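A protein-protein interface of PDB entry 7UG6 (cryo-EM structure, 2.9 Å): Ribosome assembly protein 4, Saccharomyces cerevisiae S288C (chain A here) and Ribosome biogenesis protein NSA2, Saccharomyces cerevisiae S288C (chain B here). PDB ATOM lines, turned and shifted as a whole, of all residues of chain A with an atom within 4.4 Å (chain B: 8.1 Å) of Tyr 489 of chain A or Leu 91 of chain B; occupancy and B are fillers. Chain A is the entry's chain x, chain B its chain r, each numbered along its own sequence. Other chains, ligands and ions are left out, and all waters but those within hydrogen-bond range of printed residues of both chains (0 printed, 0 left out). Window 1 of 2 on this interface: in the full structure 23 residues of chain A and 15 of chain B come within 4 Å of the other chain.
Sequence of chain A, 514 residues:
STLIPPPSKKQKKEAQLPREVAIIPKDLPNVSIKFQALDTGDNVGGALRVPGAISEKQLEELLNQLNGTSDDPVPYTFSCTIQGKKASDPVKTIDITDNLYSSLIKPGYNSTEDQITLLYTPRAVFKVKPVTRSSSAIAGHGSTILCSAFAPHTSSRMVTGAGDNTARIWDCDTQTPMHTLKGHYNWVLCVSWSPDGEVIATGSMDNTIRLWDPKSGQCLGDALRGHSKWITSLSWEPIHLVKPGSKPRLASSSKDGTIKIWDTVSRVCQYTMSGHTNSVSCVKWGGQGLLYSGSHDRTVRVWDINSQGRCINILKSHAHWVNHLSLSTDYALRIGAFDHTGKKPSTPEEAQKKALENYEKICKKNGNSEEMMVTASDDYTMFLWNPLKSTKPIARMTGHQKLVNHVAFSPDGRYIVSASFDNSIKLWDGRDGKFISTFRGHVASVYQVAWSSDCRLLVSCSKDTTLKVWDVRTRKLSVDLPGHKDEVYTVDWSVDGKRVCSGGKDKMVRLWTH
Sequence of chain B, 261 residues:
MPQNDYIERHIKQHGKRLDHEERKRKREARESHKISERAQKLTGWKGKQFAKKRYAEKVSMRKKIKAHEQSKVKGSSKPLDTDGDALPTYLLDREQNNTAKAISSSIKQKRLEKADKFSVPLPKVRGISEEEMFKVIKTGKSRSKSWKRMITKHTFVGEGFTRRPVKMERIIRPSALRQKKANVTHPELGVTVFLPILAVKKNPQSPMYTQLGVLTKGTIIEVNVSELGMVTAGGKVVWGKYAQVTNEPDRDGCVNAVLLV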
ATOM      1  N   ILE A 145      15.947 -19.509   8.186  1.00  0.00           N
ATOM      2  CA  ILE A 145      17.144 -18.681   8.158  1.00  0.00           C
ATOM      3  C   ILE A 145      17.019 -17.590   9.207  1.00  0.00           C
ATOM      4  O   ILE A 145      15.978 -16.933   9.313  1.00  0.00           O
ATOM      5  CB  ILE A 145      17.333 -18.084   6.764  1.00  0.00           C
ATOM      6  CG1 ILE A 145      17.691 -19.190   5.803  1.00  0.00           C
ATOM      7  CG2 ILE A 145      18.425 -17.055   6.764  1.00  0.00           C
ATOM      8  CD1 ILE A 145      17.909 -18.686   4.467  1.00  0.00           C
ATOM      9  N   PHE A 421       7.938  -2.517  14.246  1.00  0.00           N
ATOM     10  CA  PHE A 421       6.655  -3.167  14.161  1.00  0.00           C
ATOM     11  C   PHE A 421       5.644  -2.031  14.176  1.00  0.00           C
ATOM     12  O   PHE A 421       5.944  -0.957  14.692  1.00  0.00           O
ATOM     13  CB  PHE A 421       6.415  -4.097  15.348  1.00  0.00           C
ATOM     14  CG  PHE A 421       7.419  -5.213  15.486  1.00  0.00           C
ATOM     15  CD1 PHE A 421       8.350  -5.482  14.517  1.00  0.00           C
ATOM     16  CD2 PHE A 421       7.365  -6.052  16.571  1.00  0.00           C
ATOM     17  CE1 PHE A 421       9.250  -6.508  14.673  1.00  0.00           C
ATOM     18  CE2 PHE A 421       8.257  -7.081  16.724  1.00  0.00           C
ATOM     19  CZ  PHE A 421       9.192  -7.312  15.772  1.00  0.00           C
ATOM     20  N   TYR A 447      11.124  -6.110   9.990  1.00  0.00           N
ATOM     21  CA  TYR A 447      12.148  -6.655  10.865  1.00  0.00           C
ATOM     22  C   TYR A 447      13.489  -5.951  10.691  1.00  0.00           C
ATOM     23  O   TYR A 447      14.008  -5.362  11.642  1.00  0.00           O
ATOM     24  CB  TYR A 447      12.295  -8.152  10.628  1.00  0.00           C
ATOM     25  CG  TYR A 447      11.124  -8.970  11.101  1.00  0.00           C
ATOM     26  CD1 TYR A 447      10.216  -8.460  12.002  1.00  0.00           C
ATOM     27  CD2 TYR A 447      10.938 -10.265  10.657  1.00  0.00           C
ATOM     28  CE1 TYR A 447       9.159  -9.209  12.439  1.00  0.00           C
ATOM     29  CE2 TYR A 447       9.886 -11.016  11.090  1.00  0.00           C
ATOM     30  CZ  TYR A 447       9.002 -10.485  11.981  1.00  0.00           C
ATOM     31  OH  TYR A 447       7.944 -11.242  12.415  1.00  0.00           O
ATOM     32  N   GLN A 448      14.059  -5.986   9.491  1.00  0.00           N
ATOM     33  CA  GLN A 448      15.394  -5.455   9.265  1.00  0.00           C
ATOM     34  C   GLN A 448      15.403  -4.489   8.093  1.00  0.00           C
ATOM     35  O   GLN A 448      14.514  -4.501   7.242  1.00  0.00           O
ATOM     36  CB  GLN A 448      16.402  -6.568   9.010  1.00  0.00           C
ATOM     37  CG  GLN A 448      16.507  -7.566  10.126  1.00  0.00           C
ATOM     38  CD  GLN A 448      17.795  -8.339  10.073  1.00  0.00           C
ATOM     39  OE1 GLN A 448      18.471  -8.359   9.051  1.00  0.00           O
ATOM     40  NE2 GLN A 448      18.149  -8.978  11.176  1.00  0.00           N
ATOM     41  N   CYS A 461      12.893  -6.016   5.104  1.00  0.00           N
ATOM     42  CA  CYS A 461      12.262  -7.319   5.142  1.00  0.00           C
ATOM     43  C   CYS A 461      11.212  -7.294   6.236  1.00  0.00           C
ATOM     44  O   CYS A 461      11.418  -6.686   7.287  1.00  0.00           O
ATOM     45  CB  CYS A 461      13.290  -8.413   5.381  1.00  0.00           C
ATOM     46  SG  CYS A 461      13.982  -8.457   7.012  1.00  0.00           S
ATOM     47  N   GLU A 487       7.519 -15.343   5.892  1.00  0.00           N
ATOM     48  CA  GLU A 487       8.103 -14.126   6.426  1.00  0.00           C
ATOM     49  C   GLU A 487       9.617 -14.163   6.355  1.00  0.00           C
ATOM     50  O   GLU A 487      10.239 -15.223   6.387  1.00  0.00           O
ATOM     51  CB  GLU A 487       7.633 -13.928   7.857  1.00  0.00           C
ATOM     52  CG  GLU A 487       8.109 -14.977   8.797  1.00  0.00           C
ATOM     53  CD  GLU A 487       7.559 -14.785  10.188  1.00  0.00           C
ATOM     54  OE1 GLU A 487       6.785 -13.832  10.391  1.00  0.00           O
ATOM     55  OE2 GLU A 487       7.896 -15.593  11.079  1.00  0.00           O
ATOM     56  N   VAL A 488      10.209 -12.980   6.233  1.00  0.00           N
ATOM     57  CA  VAL A 488      11.631 -12.821   5.964  1.00  0.00           C
ATOM     58  C   VAL A 488      12.296 -12.141   7.146  1.00  0.00           C
ATOM     59  O   VAL A 488      11.854 -11.083   7.605  1.00  0.00           O
ATOM     60  CB  VAL A 488      11.862 -12.050   4.659  1.00  0.00           C
ATOM     61  CG1 VAL A 488      11.446 -12.896   3.542  1.00  0.00           C
ATOM     62  CG2 VAL A 488      10.977 -10.864   4.619  1.00  0.00           C
ATOM     63  N   TYR A 489      13.353 -12.763   7.646  1.00  0.00           N
ATOM     64  CA  TYR A 489      14.017 -12.332   8.859  1.00  0.00           C
ATOM     65  C   TYR A 489      15.283 -11.546   8.604  1.00  0.00           C
ATOM     66  O   TYR A 489      15.676 -10.736   9.447  1.00  0.00           O
ATOM     67  CB  TYR A 489      14.372 -13.543   9.705  1.00  0.00           C
ATOM     68  CG  TYR A 489      13.188 -14.304  10.213  1.00  0.00           C
ATOM     69  CD1 TYR A 489      13.188 -15.682  10.219  1.00  0.00           C
ATOM     70  CD2 TYR A 489      12.087 -13.648  10.717  1.00  0.00           C
ATOM     71  CE1 TYR A 489      12.122 -16.380  10.692  1.00  0.00           C
ATOM     72  CE2 TYR A 489      11.017 -14.342  11.194  1.00  0.00           C
ATOM     73  CZ  TYR A 489      11.041 -15.708  11.178  1.00  0.00           C
ATOM     74  OH  TYR A 489       9.970 -16.412  11.652  1.00  0.00           O
ATOM     75  N   THR A 490      15.943 -11.781   7.482  1.00  0.00           N
ATOM     76  CA  THR A 490      17.246 -11.204   7.208  1.00  0.00           C
ATOM     77  C   THR A 490      17.224 -10.493   5.868  1.00  0.00           C
ATOM     78  O   THR A 490      16.533 -10.904   4.937  1.00  0.00           O
ATOM     79  CB  THR A 490      18.331 -12.263   7.160  1.00  0.00           C
ATOM     80  OG1 THR A 490      18.253 -12.949   5.911  1.00  0.00           O
ATOM     81  CG2 THR A 490      18.119 -13.270   8.252  1.00  0.00           C
ATOM     82  N   GLY A 503      16.182 -14.051   3.673  1.00  0.00           N
ATOM     83  CA  GLY A 503      15.950 -15.358   4.233  1.00  0.00           C
ATOM     84  C   GLY A 503      14.936 -15.250   5.337  1.00  0.00           C
ATOM     85  O   GLY A 503      14.778 -14.197   5.957  1.00  0.00           O
ATOM     86  N   GLY A 504      14.241 -16.347   5.568  1.00  0.00           N
ATOM     87  CA  GLY A 504      13.243 -16.325   6.605  1.00  0.00           C
ATOM     88  C   GLY A 504      12.655 -17.680   6.884  1.00  0.00           C
ATOM     89  O   GLY A 504      13.341 -18.697   6.790  1.00  0.00           O
ATOM     90  N   LYS A 505      11.371 -17.703   7.223  1.00  0.00           N
ATOM     91  CA  LYS A 505      10.699 -18.952   7.521  1.00  0.00           C
ATOM     92  C   LYS A 505      10.579 -19.849   6.302  1.00  0.00           C
ATOM     93  O   LYS A 505      10.290 -21.038   6.455  1.00  0.00           O
ATOM     94  CB  LYS A 505       9.321 -18.651   8.101  1.00  0.00           C
ATOM     95  CG  LYS A 505       8.764 -19.724   9.000  1.00  0.00           C
ATOM     96  CD  LYS A 505       7.539 -19.231   9.731  1.00  0.00           C
ATOM     97  CE  LYS A 505       6.728 -20.390  10.255  1.00  0.00           C
ATOM     98  NZ  LYS A 505       5.462 -19.955  10.897  1.00  0.00           N
ATOM     99  N   ASP B  85      11.456 -24.546  14.118  1.00  0.00           N
ATOM    100  CA  ASP B  85      10.796 -23.342  14.597  1.00  0.00           C
ATOM    101  C   ASP B  85      11.796 -22.406  15.250  1.00  0.00           C
ATOM    102  O   ASP B  85      11.631 -22.004  16.400  1.00  0.00           O
ATOM    103  CB  ASP B  85       9.679 -23.694  15.579  1.00  0.00           C
ATOM    104  CG  ASP B  85       8.609 -22.627  15.650  1.00  0.00           C
ATOM    105  OD1 ASP B  85       8.341 -21.978  14.618  1.00  0.00           O
ATOM    106  OD2 ASP B  85       8.028 -22.441  16.734  1.00  0.00           O
ATOM    107  N   ALA B  86      12.839 -22.065  14.504  1.00  0.00           N
ATOM    108  CA  ALA B  86      13.829 -21.124  14.992  1.00  0.00           C
ATOM    109  C   ALA B  86      13.336 -19.693  14.815  1.00  0.00           C
ATOM    110  O   ALA B  86      12.471 -19.405  13.987  1.00  0.00           O
ATOM    111  CB  ALA B  86      15.153 -21.328  14.267  1.00  0.00           C
ATOM    112  N   LEU B  87      13.891 -18.793  15.614  1.00  0.00           N
ATOM    113  CA  LEU B  87      13.508 -17.396  15.607  1.00  0.00           C
ATOM    114  C   LEU B  87      14.763 -16.539  15.610  1.00  0.00           C
ATOM    115  O   LEU B  87      15.802 -16.965  16.114  1.00  0.00           O
ATOM    116  CB  LEU B  87      12.654 -17.062  16.835  1.00  0.00           C
ATOM    117  CG  LEU B  87      11.277 -17.715  16.959  1.00  0.00           C
ATOM    118  CD1 LEU B  87      10.642 -17.382  18.296  1.00  0.00           C
ATOM    119  CD2 LEU B  87      10.353 -17.316  15.828  1.00  0.00           C
ATOM    120  N   PRO B  88      14.702 -15.339  15.047  1.00  0.00           N
ATOM    121  CA  PRO B  88      15.855 -14.443  15.082  1.00  0.00           C
ATOM    122  C   PRO B  88      16.034 -13.829  16.455  1.00  0.00           C
ATOM    123  O   PRO B  88      15.116 -13.767  17.270  1.00  0.00           O
ATOM    124  CB  PRO B  88      15.503 -13.363  14.064  1.00  0.00           C
ATOM    125  CG  PRO B  88      14.403 -13.875  13.327  1.00  0.00           C
ATOM    126  CD  PRO B  88      13.647 -14.791  14.202  1.00  0.00           C
ATOM    127  N   THR B  89      17.225 -13.272  16.659  1.00  0.00           N
ATOM    128  CA  THR B  89      17.604 -12.771  17.971  1.00  0.00           C
ATOM    129  C   THR B  89      16.685 -11.663  18.454  1.00  0.00           C
ATOM    130  O   THR B  89      16.669 -11.355  19.648  1.00  0.00           O
ATOM    131  CB  THR B  89      19.036 -12.269  17.933  1.00  0.00           C
ATOM    132  OG1 THR B  89      19.374 -11.726  19.212  1.00  0.00           O
ATOM    133  CG2 THR B  89      19.172 -11.191  16.884  1.00  0.00           C
ATOM    134  N   TYR B  90      15.932 -11.041  17.560  1.00  0.00           N
ATOM    135  CA  TYR B  90      14.969 -10.037  17.974  1.00  0.00           C
ATOM    136  C   TYR B  90      13.581 -10.609  18.207  1.00  0.00           C
ATOM    137  O   TYR B  90      12.688  -9.863  18.615  1.00  0.00           O
ATOM    138  CB  TYR B  90      14.893  -8.908  16.946  1.00  0.00           C
ATOM    139  CG  TYR B  90      14.800  -9.384  15.521  1.00  0.00           C
ATOM    140  CD1 TYR B  90      15.923  -9.457  14.727  1.00  0.00           C
ATOM    141  CD2 TYR B  90      13.594  -9.774  14.974  1.00  0.00           C
ATOM    142  CE1 TYR B  90      15.849  -9.897  13.434  1.00  0.00           C
ATOM    143  CE2 TYR B  90      13.514 -10.213  13.683  1.00  0.00           C
ATOM    144  CZ  TYR B  90      14.643 -10.273  12.919  1.00  0.00           C
ATOM    145  OH  TYR B  90      14.573 -10.715  11.627  1.00  0.00           O
ATOM    146  N   LEU B  91      13.367 -11.901  17.960  1.00  0.00           N
ATOM    147  CA  LEU B  91      12.078 -12.507  18.245  1.00  0.00           C
ATOM    148  C   LEU B  91      12.102 -13.507  19.379  1.00  0.00           C
ATOM    149  O   LEU B  91      11.048 -14.057  19.710  1.00  0.00           O
ATOM    150  CB  LEU B  91      11.490 -13.197  17.007  1.00  0.00           C
ATOM    151  CG  LEU B  91      11.098 -12.277  15.862  1.00  0.00           C
ATOM    152  CD1 LEU B  91      10.616 -13.085  14.690  1.00  0.00           C
ATOM    153  CD2 LEU B  91      10.045 -11.310  16.315  1.00  0.00           C
ATOM    154  N   LEU B  92      13.250 -13.771  19.977  1.00  0.00           N
ATOM    155  CA  LEU B  92      13.277 -14.535  21.208  1.00  0.00           C
ATOM    156  C   LEU B  92      12.893 -13.640  22.375  1.00  0.00           C
ATOM    157  O   LEU B  92      13.252 -12.460  22.408  1.00  0.00           O
ATOM    158  CB  LEU B  92      14.651 -15.153  21.428  1.00  0.00           C
ATOM    159  CG  LEU B  92      15.005 -16.405  20.627  1.00  0.00           C
ATOM    160  CD1 LEU B  92      15.234 -16.144  19.190  1.00  0.00           C
ATOM    161  CD2 LEU B  92      16.251 -16.963  21.188  1.00  0.00           C
ATOM    162  N   ASP B  93      12.155 -14.217  23.324  1.00  0.00           N
ATOM    163  CA  ASP B  93      11.503 -13.531  24.439  1.00  0.00           C
ATOM    164  C   ASP B  93      10.348 -12.649  23.991  1.00  0.00           C
ATOM    165  O   ASP B  93      10.190 -11.536  24.497  1.00  0.00           O
ATOM    166  CB  ASP B  93      12.492 -12.699  25.267  1.00  0.00           C
ATOM    167  CG  ASP B  93      13.764 -13.454  25.584  1.00  0.00           C
ATOM    168  OD1 ASP B  93      13.685 -14.674  25.840  1.00  0.00           O
ATOM    169  OD2 ASP B  93      14.844 -12.829  25.568  1.00  0.00           O
ATOM    170  N   ARG B  94       9.518 -13.123  23.062  1.00  0.00           N
ATOM    171  CA  ARG B  94       8.475 -12.287  22.485  1.00  0.00           C
ATOM    172  C   ARG B  94       7.090 -12.919  22.470  1.00  0.00           C
ATOM    173  O   ARG B  94       6.100 -12.189  22.577  1.00  0.00           O
ATOM    174  CB  ARG B  94       8.835 -11.921  21.045  1.00  0.00           C
ATOM    175  CG  ARG B  94       9.930 -10.928  20.916  1.00  0.00           C
ATOM    176  CD  ARG B  94       9.455  -9.601  21.403  1.00  0.00           C
ATOM    177  NE  ARG B  94       9.993  -8.506  20.617  1.00  0.00           N
ATOM    178  CZ  ARG B  94      11.253  -8.107  20.659  1.00  0.00           C
ATOM    179  NH1 ARG B  94      12.123  -8.710  21.447  1.00  0.00           N
ATOM    180  NH2 ARG B  94      11.644  -7.099  19.906  1.00  0.00           N
ATOM    181  N   GLU B  95       6.993 -14.237  22.331  1.00  0.00           N
ATOM    182  CA  GLU B  95       5.738 -14.861  21.934  1.00  0.00           C
ATOM    183  C   GLU B  95       4.670 -14.714  23.013  1.00  0.00           C
ATOM    184  O   GLU B  95       4.963 -14.637  24.209  1.00  0.00           O
ATOM    185  CB  GLU B  95       5.960 -16.339  21.611  1.00  0.00           C
ATOM    186  CG  GLU B  95       4.902 -16.949  20.700  1.00  0.00           C
ATOM    187  CD  GLU B  95       5.222 -18.380  20.306  1.00  0.00           C
ATOM    188  OE1 GLU B  95       5.762 -19.126  21.147  1.00  0.00           O
ATOM    189  OE2 GLU B  95       4.944 -18.753  19.151  1.00  0.00           O
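O of Tyr 489 of chain A sits at hydrogen-bond distance from OH of Tyr 90 of chain B, 2.4 Å away.
Phe 421 of chain A touches none of the printed residues of chain B.
Printed residues of chain B within 4 Å of Tyr 447 of chain A: Tyr 90 and Leu 91.
Printed residues of chain B within 4 Å of Gln 448 of chain A: Tyr 90 (3.4 Å).
Of chain B, only Pro 88 (3.4 Å), Tyr 90 (2.4 Å) and Leu 91 (3.7 Å) come within 4 Å of Tyr 489 of chain A.
Printed residues of chain A within 4 Å of Pro 88 of chain B: Tyr 489 (3.4 Å).
Leu 91 of chain B touches just these residues of chain A: Tyr 447 (3.96 Å) and Tyr 489 (3.7 Å).
The backbone carbonyl oxygen (O) of Tyr 90 of chain B lies close to the guanidinium group (NH1) of Arg 94 of chain B, at 3.1 Å.
The backbone NH (N) of Tyr 447 of chain A lies within hydrogen-bond range of the backbone carbonyl oxygen (O) of Cys 461 of chain A, at 2.8 Å.
The side-chain hydroxyl of Tyr 447 of chain A sits at hydrogen-bond distance from the side-chain carboxylate of Glu 487 of chain A, at 3.5 Å.
N of Cys 461 of chain A lies within hydrogen-bond range of O of Gln 448 of chain A, 3.1 Å away.
SG of Cys 461 of chain A sits close to O of Tyr 489 of chain A (3.7 Å).
The backbone carbonyl oxygen (O) of Gly 503 of chain A lies within hydrogen-bond range of the backbone NH (N) of Tyr 489 of chain A (2.6 Å).
Printed residues of chain B that touch a printed residue of chain A: Pro 88, Tyr 90 and Leu 91.
Hydrophobic or aromatic side chains of chain A within 4 Å of the printed part of chain B: Tyr 447 and Tyr 489.
Among the printed residues, 6 pairs touch across the chains.
Among the printed residues, pairs that only touch across the chains: Gln 448 of chain A with Tyr 90 of chain B (3.4 Å), Tyr 489 of chain A with Pro 88 of chain B (3.4 Å), Tyr 447 of chain A with Tyr 90 of chain B (3.6 Å), Tyr 489 of chain A with Leu 91 of chain B (3.7 Å) and Tyr 447 of chain A with Leu 91 of chain B (3.96 Å).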
